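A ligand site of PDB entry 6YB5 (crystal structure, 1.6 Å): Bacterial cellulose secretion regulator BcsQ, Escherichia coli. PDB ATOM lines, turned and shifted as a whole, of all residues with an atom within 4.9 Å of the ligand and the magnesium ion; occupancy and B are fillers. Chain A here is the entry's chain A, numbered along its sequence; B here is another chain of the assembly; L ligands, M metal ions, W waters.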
ATOM      1  N   ARG A  10     -14.698 -32.371  39.581  1.00  0.00           N
ATOM      2  CA  ARG A  10     -14.923 -33.565  38.778  1.00  0.00           C
ATOM      3  C   ARG A  10     -14.055 -33.405  37.532  1.00  0.00           C
ATOM      4  O   ARG A  10     -13.667 -32.285  37.190  1.00  0.00           O
ATOM      5  CB  ARG A  10     -16.411 -33.686  38.418  1.00  0.00           C
ATOM      6  CG  ARG A  10     -16.797 -34.716  37.382  1.00  0.00           C
ATOM      7  CD  ARG A  10     -18.269 -34.602  37.102  1.00  0.00           C
ATOM      8  NE  ARG A  10     -18.612 -33.626  36.062  1.00  0.00           N
ATOM      9  CZ  ARG A  10     -19.698 -32.871  36.113  1.00  0.00           C
ATOM     10  NH1 ARG A  10     -20.506 -32.946  37.153  1.00  0.00           N
ATOM     11  NH2 ARG A  10     -19.987 -32.021  35.134  1.00  0.00           N
ATOM     12  N   GLY A  11     -13.761 -34.510  36.868  1.00  0.00           N
ATOM     13  CA  GLY A  11     -13.140 -34.396  35.553  1.00  0.00           C
ATOM     14  C   GLY A  11     -14.042 -33.693  34.557  1.00  0.00           C
ATOM     15  O   GLY A  11     -15.278 -33.691  34.678  1.00  0.00           O
ATOM     16  N   GLY A  12     -13.423 -33.077  33.558  1.00  0.00           N
ATOM     17  CA  GLY A  12     -14.141 -32.537  32.421  1.00  0.00           C
ATOM     18  C   GLY A  12     -14.887 -31.234  32.635  1.00  0.00           C
ATOM     19  O   GLY A  12     -15.629 -30.815  31.738  1.00  0.00           O
ATOM     20  N   VAL A  13     -14.725 -30.576  33.782  1.00  0.00           N
ATOM     21  CA  VAL A  13     -15.508 -29.369  34.054  1.00  0.00           C
ATOM     22  C   VAL A  13     -14.928 -28.110  33.416  1.00  0.00           C
ATOM     23  O   VAL A  13     -15.592 -27.061  33.441  1.00  0.00           O
ATOM     24  CB  VAL A  13     -15.672 -29.142  35.569  1.00  0.00           C
ATOM     25  CG1 VAL A  13     -16.593 -30.231  36.164  1.00  0.00           C
ATOM     26  CG2 VAL A  13     -14.305 -29.107  36.279  1.00  0.00           C
ATOM     27  N   GLY A  14     -13.717 -28.183  32.835  1.00  0.00           N
ATOM     28  CA  GLY A  14     -13.110 -27.047  32.159  1.00  0.00           C
ATOM     29  C   GLY A  14     -11.841 -26.512  32.792  1.00  0.00           C
ATOM     30  O   GLY A  14     -11.368 -25.444  32.404  1.00  0.00           O
ATOM     31  N   THR A  15     -11.256 -27.267  33.727  1.00  0.00           N
ATOM     32  CA  THR A  15     -10.107 -26.777  34.506  1.00  0.00           C
ATOM     33  C   THR A  15      -8.953 -26.351  33.620  1.00  0.00           C
ATOM     34  O   THR A  15      -8.361 -25.278  33.808  1.00  0.00           O
ATOM     35  CB  THR A  15      -9.671 -27.857  35.492  1.00  0.00           C
ATOM     36  OG1 THR A  15     -10.801 -28.232  36.278  1.00  0.00           O
ATOM     37  CG2 THR A  15      -8.572 -27.324  36.414  1.00  0.00           C
ATOM     38  N   THR A  16      -8.598 -27.192  32.652  1.00  0.00           N
ATOM     39  CA  THR A  16      -7.414 -26.908  31.828  1.00  0.00           C
ATOM     40  C   THR A  16      -7.647 -25.710  30.913  1.00  0.00           C
ATOM     41  O   THR A  16      -6.756 -24.871  30.763  1.00  0.00           O
ATOM     42  CB  THR A  16      -7.033 -28.152  31.039  1.00  0.00           C
ATOM     43  OG1 THR A  16      -6.720 -29.205  31.945  1.00  0.00           O
ATOM     44  CG2 THR A  16      -5.815 -27.870  30.150  1.00  0.00           C
ATOM     45  N   THR A  17      -8.827 -25.632  30.276  1.00  0.00           N
ATOM     46  CA  THR A  17      -9.139 -24.486  29.413  1.00  0.00           C
ATOM     47  C   THR A  17      -9.099 -23.186  30.202  1.00  0.00           C
ATOM     48  O   THR A  17      -8.604 -22.165  29.720  1.00  0.00           O
ATOM     49  CB  THR A  17     -10.512 -24.689  28.765  1.00  0.00           C
ATOM     50  OG1 THR A  17     -10.512 -25.929  28.060  1.00  0.00           O
ATOM     51  CG2 THR A  17     -10.842 -23.558  27.782  1.00  0.00           C
ATOM     52  N   ILE A  18      -9.603 -23.233  31.443  1.00  0.00           N
ATOM     53  CA  ILE A  18      -9.618 -22.033  32.275  1.00  0.00           C
ATOM     54  C   ILE A  18      -8.200 -21.670  32.710  1.00  0.00           C
ATOM     55  O   ILE A  18      -7.848 -20.486  32.730  1.00  0.00           O
ATOM     56  CB  ILE A  18     -10.550 -22.252  33.480  1.00  0.00           C
ATOM     57  CG1 ILE A  18     -11.988 -22.306  32.978  1.00  0.00           C
ATOM     58  CG2 ILE A  18     -10.398 -21.112  34.504  1.00  0.00           C
ATOM     59  CD1 ILE A  18     -12.990 -22.836  33.998  1.00  0.00           C
ATOM     60  N   CYS A  39      -1.134 -32.343  35.451  1.00  0.00           N
ATOM     61  CA  CYS A  39      -1.997 -33.471  35.131  1.00  0.00           C
ATOM     62  C   CYS A  39      -1.260 -34.450  34.240  1.00  0.00           C
ATOM     63  O   CYS A  39      -0.651 -34.036  33.246  1.00  0.00           O
ATOM     64  CB  CYS A  39      -3.247 -33.017  34.407  1.00  0.00           C
ATOM     65  SG  CYS A  39      -4.244 -31.914  35.351  1.00  0.00           S
ATOM     66  N   ASP A  41      -2.333 -36.349  31.989  1.00  0.00           N
ATOM     67  CA  ASP A  41      -2.734 -36.386  30.580  1.00  0.00           C
ATOM     68  C   ASP A  41      -2.052 -35.324  29.738  1.00  0.00           C
ATOM     69  O   ASP A  41      -2.149 -35.378  28.510  1.00  0.00           O
ATOM     70  CB  ASP A  41      -4.251 -36.269  30.400  1.00  0.00           C
ATOM     71  CG  ASP A  41      -4.908 -35.452  31.464  1.00  0.00           C
ATOM     72  OD1 ASP A  41      -4.930 -34.211  31.306  1.00  0.00           O
ATOM     73  OD2 ASP A  41      -5.400 -36.054  32.438  1.00  0.00           O
ATOM     74  N   LEU A  43      -2.371 -32.197  28.809  1.00  0.00           N
ATOM     75  CA  LEU A  43      -3.190 -31.535  27.803  1.00  0.00           C
ATOM     76  C   LEU A  43      -2.970 -30.034  27.725  1.00  0.00           C
ATOM     77  O   LEU A  43      -3.263 -29.438  26.672  1.00  0.00           O
ATOM     78  CB  LEU A  43      -4.671 -31.806  28.057  1.00  0.00           C
ATOM     79  CG  LEU A  43      -5.109 -33.278  27.946  1.00  0.00           C
ATOM     80  CD1 LEU A  43      -6.530 -33.491  28.489  1.00  0.00           C
ATOM     81  CD2 LEU A  43      -5.010 -33.762  26.516  1.00  0.00           C
ATOM     82  N   ASP A 124      -2.197 -26.400  36.908  1.00  0.00           N
ATOM     83  CA  ASP A 124      -3.358 -27.211  36.545  1.00  0.00           C
ATOM     84  C   ASP A 124      -3.244 -28.544  37.272  1.00  0.00           C
ATOM     85  O   ASP A 124      -2.319 -29.327  36.992  1.00  0.00           O
ATOM     86  CB  ASP A 124      -3.371 -27.385  35.023  1.00  0.00           C
ATOM     87  CG  ASP A 124      -4.570 -28.186  34.491  1.00  0.00           C
ATOM     88  OD1 ASP A 124      -5.496 -28.564  35.255  1.00  0.00           O
ATOM     89  OD2 ASP A 124      -4.569 -28.421  33.265  1.00  0.00           O
ATOM     90  N   ASN A 171     -18.171 -22.941  35.720  1.00  0.00           N
ATOM     91  CA  ASN A 171     -17.928 -22.903  34.290  1.00  0.00           C
ATOM     92  C   ASN A 171     -19.081 -23.607  33.581  1.00  0.00           C
ATOM     93  O   ASN A 171     -19.843 -24.361  34.195  1.00  0.00           O
ATOM     94  CB  ASN A 171     -16.585 -23.582  33.933  1.00  0.00           C
ATOM     95  CG  ASN A 171     -16.260 -23.521  32.457  1.00  0.00           C
ATOM     96  OD1 ASN A 171     -16.405 -22.481  31.807  1.00  0.00           O
ATOM     97  ND2 ASN A 171     -15.803 -24.639  31.907  1.00  0.00           N
ATOM     98  N   ASN A 172     -19.198 -23.382  32.264  1.00  0.00           N
ATOM     99  CA  ASN A 172     -20.168 -24.093  31.421  1.00  0.00           C
ATOM    100  C   ASN A 172     -21.623 -23.706  31.737  1.00  0.00           C
ATOM    101  O   ASN A 172     -22.537 -24.489  31.485  1.00  0.00           O
ATOM    102  CB  ASN A 172     -20.012 -25.627  31.542  1.00  0.00           C
ATOM    103  CG  ASN A 172     -18.922 -26.193  30.636  1.00  0.00           C
ATOM    104  OD1 ASN A 172     -18.718 -25.714  29.523  1.00  0.00           O
ATOM    105  ND2 ASN A 172     -18.253 -27.246  31.098  1.00  0.00           N
ATOM    106  N   ILE A 199     -18.452 -18.425  34.406  1.00  0.00           N
ATOM    107  CA  ILE A 199     -18.096 -18.534  32.999  1.00  0.00           C
ATOM    108  C   ILE A 199     -19.216 -19.276  32.281  1.00  0.00           C
ATOM    109  O   ILE A 199     -19.580 -20.387  32.687  1.00  0.00           O
ATOM    110  CB  ILE A 199     -16.760 -19.278  32.797  1.00  0.00           C
ATOM    111  CG1 ILE A 199     -15.684 -18.645  33.685  1.00  0.00           C
ATOM    112  CG2 ILE A 199     -16.339 -19.241  31.318  1.00  0.00           C
ATOM    113  CD1 ILE A 199     -14.439 -19.465  33.733  1.00  0.00           C
ATOM    114  N   HIS A 200     -19.746 -18.669  31.222  1.00  0.00           N
ATOM    115  CA  HIS A 200     -20.829 -19.286  30.469  1.00  0.00           C
ATOM    116  C   HIS A 200     -20.300 -20.342  29.507  1.00  0.00           C
ATOM    117  O   HIS A 200     -19.154 -20.295  29.050  1.00  0.00           O
ATOM    118  CB  HIS A 200     -21.609 -18.240  29.671  1.00  0.00           C
ATOM    119  CG  HIS A 200     -22.628 -17.506  30.484  1.00  0.00           C
ATOM    120  ND1 HIS A 200     -22.317 -16.410  31.262  1.00  0.00           N
ATOM    121  CD2 HIS A 200     -23.965 -17.705  30.628  1.00  0.00           C
ATOM    122  CE1 HIS A 200     -23.419 -15.970  31.856  1.00  0.00           C
ATOM    123  NE2 HIS A 200     -24.426 -16.751  31.495  1.00  0.00           N
ATOM    124  N   ARG A 201     -21.163 -21.297  29.181  1.00  0.00           N
ATOM    125  CA  ARG A 201     -20.944 -22.103  27.992  1.00  0.00           C
ATOM    126  C   ARG A 201     -20.786 -21.186  26.785  1.00  0.00           C
ATOM    127  O   ARG A 201     -21.565 -20.248  26.573  1.00  0.00           O
ATOM    128  CB  ARG A 201     -22.122 -23.070  27.805  1.00  0.00           C
ATOM    129  CG  ARG A 201     -22.024 -23.844  26.513  1.00  0.00           C
ATOM    130  CD  ARG A 201     -22.661 -25.223  26.593  1.00  0.00           C
ATOM    131  NE  ARG A 201     -22.080 -26.086  25.575  1.00  0.00           N
ATOM    132  CZ  ARG A 201     -20.962 -26.799  25.741  1.00  0.00           C
ATOM    133  NH1 ARG A 201     -20.315 -26.749  26.901  1.00  0.00           N
ATOM    134  NH2 ARG A 201     -20.485 -27.539  24.756  1.00  0.00           N
ATOM    135  N   ASP A 202     -19.747 -21.442  25.989  1.00  0.00           N
ATOM    136  CA  ASP A 202     -19.386 -20.551  24.881  1.00  0.00           C
ATOM    137  C   ASP A 202     -18.677 -21.383  23.823  1.00  0.00           C
ATOM    138  O   ASP A 202     -17.725 -22.085  24.137  1.00  0.00           O
ATOM    139  CB  ASP A 202     -18.483 -19.416  25.398  1.00  0.00           C
ATOM    140  CG  ASP A 202     -18.251 -18.309  24.367  1.00  0.00           C
ATOM    141  OD1 ASP A 202     -18.220 -18.587  23.139  1.00  0.00           O
ATOM    142  OD2 ASP A 202     -18.111 -17.153  24.797  1.00  0.00           O
ATOM    143  N   MET A 205     -14.918 -21.470  23.748  1.00  0.00           N
ATOM    144  CA  MET A 205     -14.196 -22.356  24.648  1.00  0.00           C
ATOM    145  C   MET A 205     -14.130 -23.793  24.137  1.00  0.00           C
ATOM    146  O   MET A 205     -13.264 -24.560  24.588  1.00  0.00           O
ATOM    147  CB  MET A 205     -14.853 -22.376  26.030  1.00  0.00           C
ATOM    148  CG  MET A 205     -14.855 -21.026  26.693  1.00  0.00           C
ATOM    149  SD  MET A 205     -13.340 -20.760  27.640  1.00  0.00           S
ATOM    150  CE  MET A 205     -13.695 -21.665  29.159  1.00  0.00           C
ATOM    151  N   ALA A 206     -15.053 -24.178  23.267  1.00  0.00           N
ATOM    152  CA  ALA A 206     -14.982 -25.475  22.602  1.00  0.00           C
ATOM    153  C   ALA A 206     -14.022 -25.444  21.423  1.00  0.00           C
ATOM    154  O   ALA A 206     -13.333 -26.436  21.149  1.00  0.00           O
ATOM    155  CB  ALA A 206     -16.364 -25.904  22.137  1.00  0.00           C
ATOM    156  N   LEU A 209      -9.255 -24.913  21.835  1.00  0.00           N
ATOM    157  CA  LEU A 209      -8.302 -26.024  21.876  1.00  0.00           C
ATOM    158  C   LEU A 209      -8.097 -26.649  20.498  1.00  0.00           C
ATOM    159  O   LEU A 209      -6.979 -27.052  20.151  1.00  0.00           O
ATOM    160  CB  LEU A 209      -8.756 -27.087  22.894  1.00  0.00           C
ATOM    161  CG  LEU A 209      -7.883 -28.349  23.064  1.00  0.00           C
ATOM    162  CD1 LEU A 209      -6.396 -28.037  23.362  1.00  0.00           C
ATOM    163  CD2 LEU A 209      -8.461 -29.281  24.137  1.00  0.00           C
ATOM    164  N   ARG B  10     -12.941 -39.756  29.921  1.00  0.00           N
ATOM    165  CA  ARG B  10     -12.541 -38.802  30.934  1.00  0.00           C
ATOM    166  C   ARG B  10     -13.708 -38.632  31.882  1.00  0.00           C
ATOM    167  O   ARG B  10     -14.798 -39.159  31.654  1.00  0.00           O
ATOM    168  CB  ARG B  10     -12.097 -37.459  30.337  1.00  0.00           C
ATOM    169  CG  ARG B  10     -13.203 -36.709  29.717  1.00  0.00           C
ATOM    170  CD  ARG B  10     -12.995 -35.185  29.830  1.00  0.00           C
ATOM    171  NE  ARG B  10     -14.224 -34.531  29.412  1.00  0.00           N
ATOM    172  CZ  ARG B  10     -14.485 -34.139  28.179  1.00  0.00           C
ATOM    173  NH1 ARG B  10     -13.580 -34.297  27.227  1.00  0.00           N
ATOM    174  NH2 ARG B  10     -15.645 -33.567  27.893  1.00  0.00           N
ATOM    175  N   GLY B  11     -13.496 -37.878  32.950  1.00  0.00           N
ATOM    176  CA  GLY B  11     -14.579 -37.667  33.881  1.00  0.00           C
ATOM    177  C   GLY B  11     -15.682 -36.790  33.305  1.00  0.00           C
ATOM    178  O   GLY B  11     -15.471 -36.012  32.371  1.00  0.00           O
ATOM    179  N   ASP B 150     -15.550 -33.687  21.485  1.00  0.00           N
ATOM    180  CA  ASP B 150     -14.856 -32.431  21.748  1.00  0.00           C
ATOM    181  C   ASP B 150     -13.355 -32.678  21.609  1.00  0.00           C
ATOM    182  O   ASP B 150     -12.910 -33.815  21.469  1.00  0.00           O
ATOM    183  CB  ASP B 150     -15.239 -31.833  23.111  1.00  0.00           C
ATOM    184  CG  ASP B 150     -14.927 -32.744  24.295  1.00  0.00           C
ATOM    185  OD1 ASP B 150     -13.829 -33.333  24.350  1.00  0.00           O
ATOM    186  OD2 ASP B 150     -15.771 -32.810  25.222  1.00  0.00           O
ATOM    187  N   ALA B 151     -12.587 -31.587  21.620  1.00  0.00           N
ATOM    188  CA  ALA B 151     -11.160 -31.695  21.322  1.00  0.00           C
ATOM    189  C   ALA B 151     -10.417 -32.485  22.393  1.00  0.00           C
ATOM    190  O   ALA B 151      -9.451 -33.184  22.091  1.00  0.00           O
ATOM    191  CB  ALA B 151     -10.549 -30.297  21.158  1.00  0.00           C
ATOM    192  N   ASN B 152     -10.862 -32.398  23.647  1.00  0.00           N
ATOM    193  CA  ASN B 152     -10.227 -33.146  24.729  1.00  0.00           C
ATOM    194  C   ASN B 152     -10.356 -34.646  24.486  1.00  0.00           C
ATOM    195  O   ASN B 152      -9.359 -35.372  24.515  1.00  0.00           O
ATOM    196  CB  ASN B 152     -10.859 -32.692  26.057  1.00  0.00           C
ATOM    197  CG  ASN B 152     -10.429 -33.507  27.273  1.00  0.00           C
ATOM    198  OD1 ASN B 152     -10.362 -34.716  27.245  1.00  0.00           O
ATOM    199  ND2 ASN B 152     -10.219 -32.806  28.397  1.00  0.00           N
ATOM    200  N   ARG B 156      -7.434 -37.509  23.672  1.00  0.00           N
ATOM    201  CA  ARG B 156      -7.300 -38.682  24.534  1.00  0.00           C
ATOM    202  C   ARG B 156      -7.348 -39.976  23.731  1.00  0.00           C
ATOM    203  O   ARG B 156      -6.628 -40.928  24.051  1.00  0.00           O
ATOM    204  CB  ARG B 156      -8.397 -38.685  25.598  1.00  0.00           C
ATOM    205  CG  ARG B 156      -8.181 -37.643  26.682  1.00  0.00           C
ATOM    206  CD  ARG B 156      -9.327 -37.735  27.691  1.00  0.00           C
ATOM    207  NE  ARG B 156      -9.120 -36.848  28.831  1.00  0.00           N
ATOM    208  CZ  ARG B 156      -8.501 -37.207  29.938  1.00  0.00           C
ATOM    209  NH1 ARG B 156      -8.008 -38.442  30.058  1.00  0.00           N
ATOM    210  NH2 ARG B 156      -8.349 -36.334  30.939  1.00  0.00           N
HETATM  211  P1  LIG L   1      -9.901 -33.260  32.181  1.00  0.00           P
HETATM  212  O1  LIG L   1      -9.620 -34.036  30.940  1.00  0.00           O
HETATM  213  O2  LIG L   1     -10.663 -33.958  33.256  1.00  0.00           O
HETATM  214  O3  LIG L   1      -8.636 -32.649  32.759  1.00  0.00           O
HETATM  215  P2  LIG L   1     -10.877 -30.509  32.205  1.00  0.00           P
HETATM  216  O4  LIG L   1     -11.706 -30.318  33.382  1.00  0.00           O
HETATM  217  O5  LIG L   1      -9.459 -29.970  32.260  1.00  0.00           O
HETATM  218  O6  LIG L   1     -10.822 -32.027  31.751  1.00  0.00           O
HETATM  219  P3  LIG L   1     -11.087 -29.151  29.628  1.00  0.00           P
HETATM  220  O7  LIG L   1     -10.077 -29.949  28.900  1.00  0.00           O
HETATM  221  O8  LIG L   1     -10.690 -27.740  29.960  1.00  0.00           O
HETATM  222  O9  LIG L   1     -11.606 -29.851  30.956  1.00  0.00           O
HETATM  223  O10 LIG L   1     -12.438 -29.018  28.806  1.00  0.00           O
HETATM  224  C1  LIG L   1     -13.176 -30.195  28.397  1.00  0.00           C
HETATM  225  C2  LIG L   1     -13.888 -29.845  27.116  1.00  0.00           C
HETATM  226  O11 LIG L   1     -14.970 -28.924  27.410  1.00  0.00           O
HETATM  227  C3  LIG L   1     -12.989 -29.186  26.065  1.00  0.00           C
HETATM  228  O12 LIG L   1     -13.064 -29.826  24.788  1.00  0.00           O
HETATM  229  C4  LIG L   1     -13.428 -27.718  26.072  1.00  0.00           C
HETATM  230  O13 LIG L   1     -13.317 -27.185  24.764  1.00  0.00           O
HETATM  231  C5  LIG L   1     -14.877 -27.790  26.568  1.00  0.00           C
HETATM  232  N1  LIG L   1     -15.289 -26.614  27.357  1.00  0.00           N
HETATM  233  C6  LIG L   1     -14.708 -26.189  28.529  1.00  0.00           C
HETATM  234  N2  LIG L   1     -15.234 -25.089  29.011  1.00  0.00           N
HETATM  235  C7  LIG L   1     -16.238 -24.767  28.108  1.00  0.00           C
HETATM  236  C8  LIG L   1     -17.155 -23.704  28.036  1.00  0.00           C
HETATM  237  N3  LIG L   1     -17.244 -22.726  28.961  1.00  0.00           N
HETATM  238  N4  LIG L   1     -17.997 -23.665  26.983  1.00  0.00           N
HETATM  239  C9  LIG L   1     -17.936 -24.647  26.081  1.00  0.00           C
HETATM  240  N5  LIG L   1     -17.130 -25.713  26.043  1.00  0.00           N
HETATM  241  C10 LIG L   1     -16.294 -25.711  27.082  1.00  0.00           C
HETATM  242 MG    MG M   1      -7.658 -30.917  32.330  1.00  0.00          MG
HETATM  243  O   HOH W   1     -14.106 -29.086  21.618  1.00  0.00           O
HETATM  244  O   HOH W   2      -7.329 -30.590  34.367  1.00  0.00           O
HETATM  245  O   HOH W   3      -6.918 -34.154  34.036  1.00  0.00           O
HETATM  246  O   HOH W   4     -16.001 -28.715  29.903  1.00  0.00           O
HETATM  247  O   HOH W   5      -9.321 -33.025  35.814  1.00  0.00           O
HETATM  248  O   HOH W   6     -11.294 -30.984  35.845  1.00  0.00           O
HETATM  249  O   HOH W   7      -5.768 -31.979  32.113  1.00  0.00           O
HETATM  250  O   HOH W   8     -11.051 -36.579  33.670  1.00  0.00           O
HETATM  251  O   HOH W   9      -8.103 -28.109  27.553  1.00  0.00           O
HETATM  252  O   HOH W  10      -7.859 -31.149  30.262  1.00  0.00           O
HETATM  253  O   HOH W  11     -17.777 -28.508  24.341  1.00  0.00           O
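N of Thr 16 lies within hydrogen-bond range of O8 of the ligand (3.5 Å).
An oxygen (O1) of the ligand lies within salt-bridge range of the guanidinium group of Arg 156 of chain B (2.6 Å).
N of Thr 17 lies within hydrogen-bond range of O8 of the ligand, 2.8 Å away.
O8 of the ligand sits at hydrogen-bond distance from OG1 of Thr 17 (2.6 Å).
The backbone carbonyl oxygen (O) of Met 205 is in hydrogen-bond range of an oxygen (O13) of the ligand (2.6 Å).
The side-chain amide nitrogen (ND2) of Asn 152 of chain B lies within hydrogen-bond range of an oxygen (O1) of the ligand (2.9 Å).
O2 of the ligand lies within hydrogen-bond range of N of Gly 12 (2.9 Å).
A nitrogen (N4) of the ligand sits close to the side-chain amide oxygen of Asn 172 (3.3 Å).
The side-chain amide oxygen (OD1) of Asn 171 sits at hydrogen-bond distance from a nitrogen (N3) of the ligand (3.0 Å).
The backbone NH (N) of Gly 14 is in hydrogen-bond range of an oxygen (O4) of the ligand, at 3.0 Å.
N4 of the ligand sits at hydrogen-bond distance from N of Asp 202 (3.0 Å).
An oxygen (O4) of the ligand is in hydrogen-bond range of the backbone NH of Val 13 (3.1 Å).
O of His 200 lies within hydrogen-bond range of N3 of the ligand.
O4 of the ligand sits at hydrogen-bond distance from N of Thr 15, 3.1 Å away.
The guanidinium group of Arg 201 sits close to a nitrogen (N5) of the ligand (3.5 Å).
The side-chain hydroxyl of Thr 16 lies close to the side-chain carboxylate of Asp 124 (2.6 Å).
The guanidinium group of Arg 156 of chain B lies within salt-bridge range of the side-chain carboxylate of Asp 41, at 3.3 Å.
The backbone NH (N) of Asn 152 of chain B lies within hydrogen-bond range of the side-chain carboxylate (OD1) of Asp 150 of chain B.
The guanidinium group (NH1) of Arg 10 of chain B is in hydrogen-bond range of the side-chain amide oxygen (OD1) of Asn 152 of chain B (3.2 Å).
The guanidinium group (NH1) of Arg 201 sits at hydrogen-bond distance from the side-chain amide oxygen (OD1) of Asn 172 (3.2 Å).
The backbone NH (N) of Asn 172 sits at hydrogen-bond distance from the backbone carbonyl oxygen (O) of Ile 199.
ND2 of Asn 171 is in hydrogen-bond range of O of Val 13 (2.9 Å).
The side-chain carboxylate (OD2) of Asp 150 of chain B is in salt-bridge range of the guanidinium group (NH2) of Arg 10 of chain B, 2.8 Å away.
Merely in contact with the ligand: Gly 11 of chain A, Leu 43, Ala 206, Arg 10 of chain B, Asp 150 of chain B and Ala 151 of chain B.
Hydrophobic or aromatic side chains within 4 Å of the ligand: Leu 43, Met 205 and Ala 206.
Of the 28 residues printed, 20 come within 4 Å of the ligand.
One residue has an atom within 4 Å of the magnesium ion: Thr 16.
The magnesium ion is bound by the side-chain hydroxyl of Thr 16 (2.0 Å), an oxygen (O3) of the ligand (2.0 Å), an oxygen (O5) of the ligand (2.0 Å), water W2 (2.1 Å), water W10 (2.1 Å) and water W7 (2.2 Å).
Water W2 lies within hydrogen-bond range of OD1 of Asp 124 (2.9 Å) and SG of Cys 39 (3.5 Å).
Water W6 lies within hydrogen-bond range of an oxygen (O4) of the ligand (2.6 Å), the side-chain hydroxyl of Thr 15 (2.8 Å) and the backbone carbonyl oxygen of Arg 10 of chain A (3.0 Å).
Water W4 lies within hydrogen-bond range of an oxygen (O11) of the ligand (2.7 Å), the backbone carbonyl oxygen (O) of Gly 12 (2.8 Å) and the side-chain amide nitrogen (ND2) of Asn 172 (2.9 Å).
Water W9 bridges O7 of the ligand and OG1 of Thr 17.
Water W11 bridges NH2 of Arg 201 and N5 of the ligand.
Water W1 lies within hydrogen-bond range of the backbone carbonyl oxygen of Ala 206 (2.8 Å), the backbone NH of Ala 151 of chain B (2.9 Å) and an oxygen (O12) of the ligand (3.4 Å).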
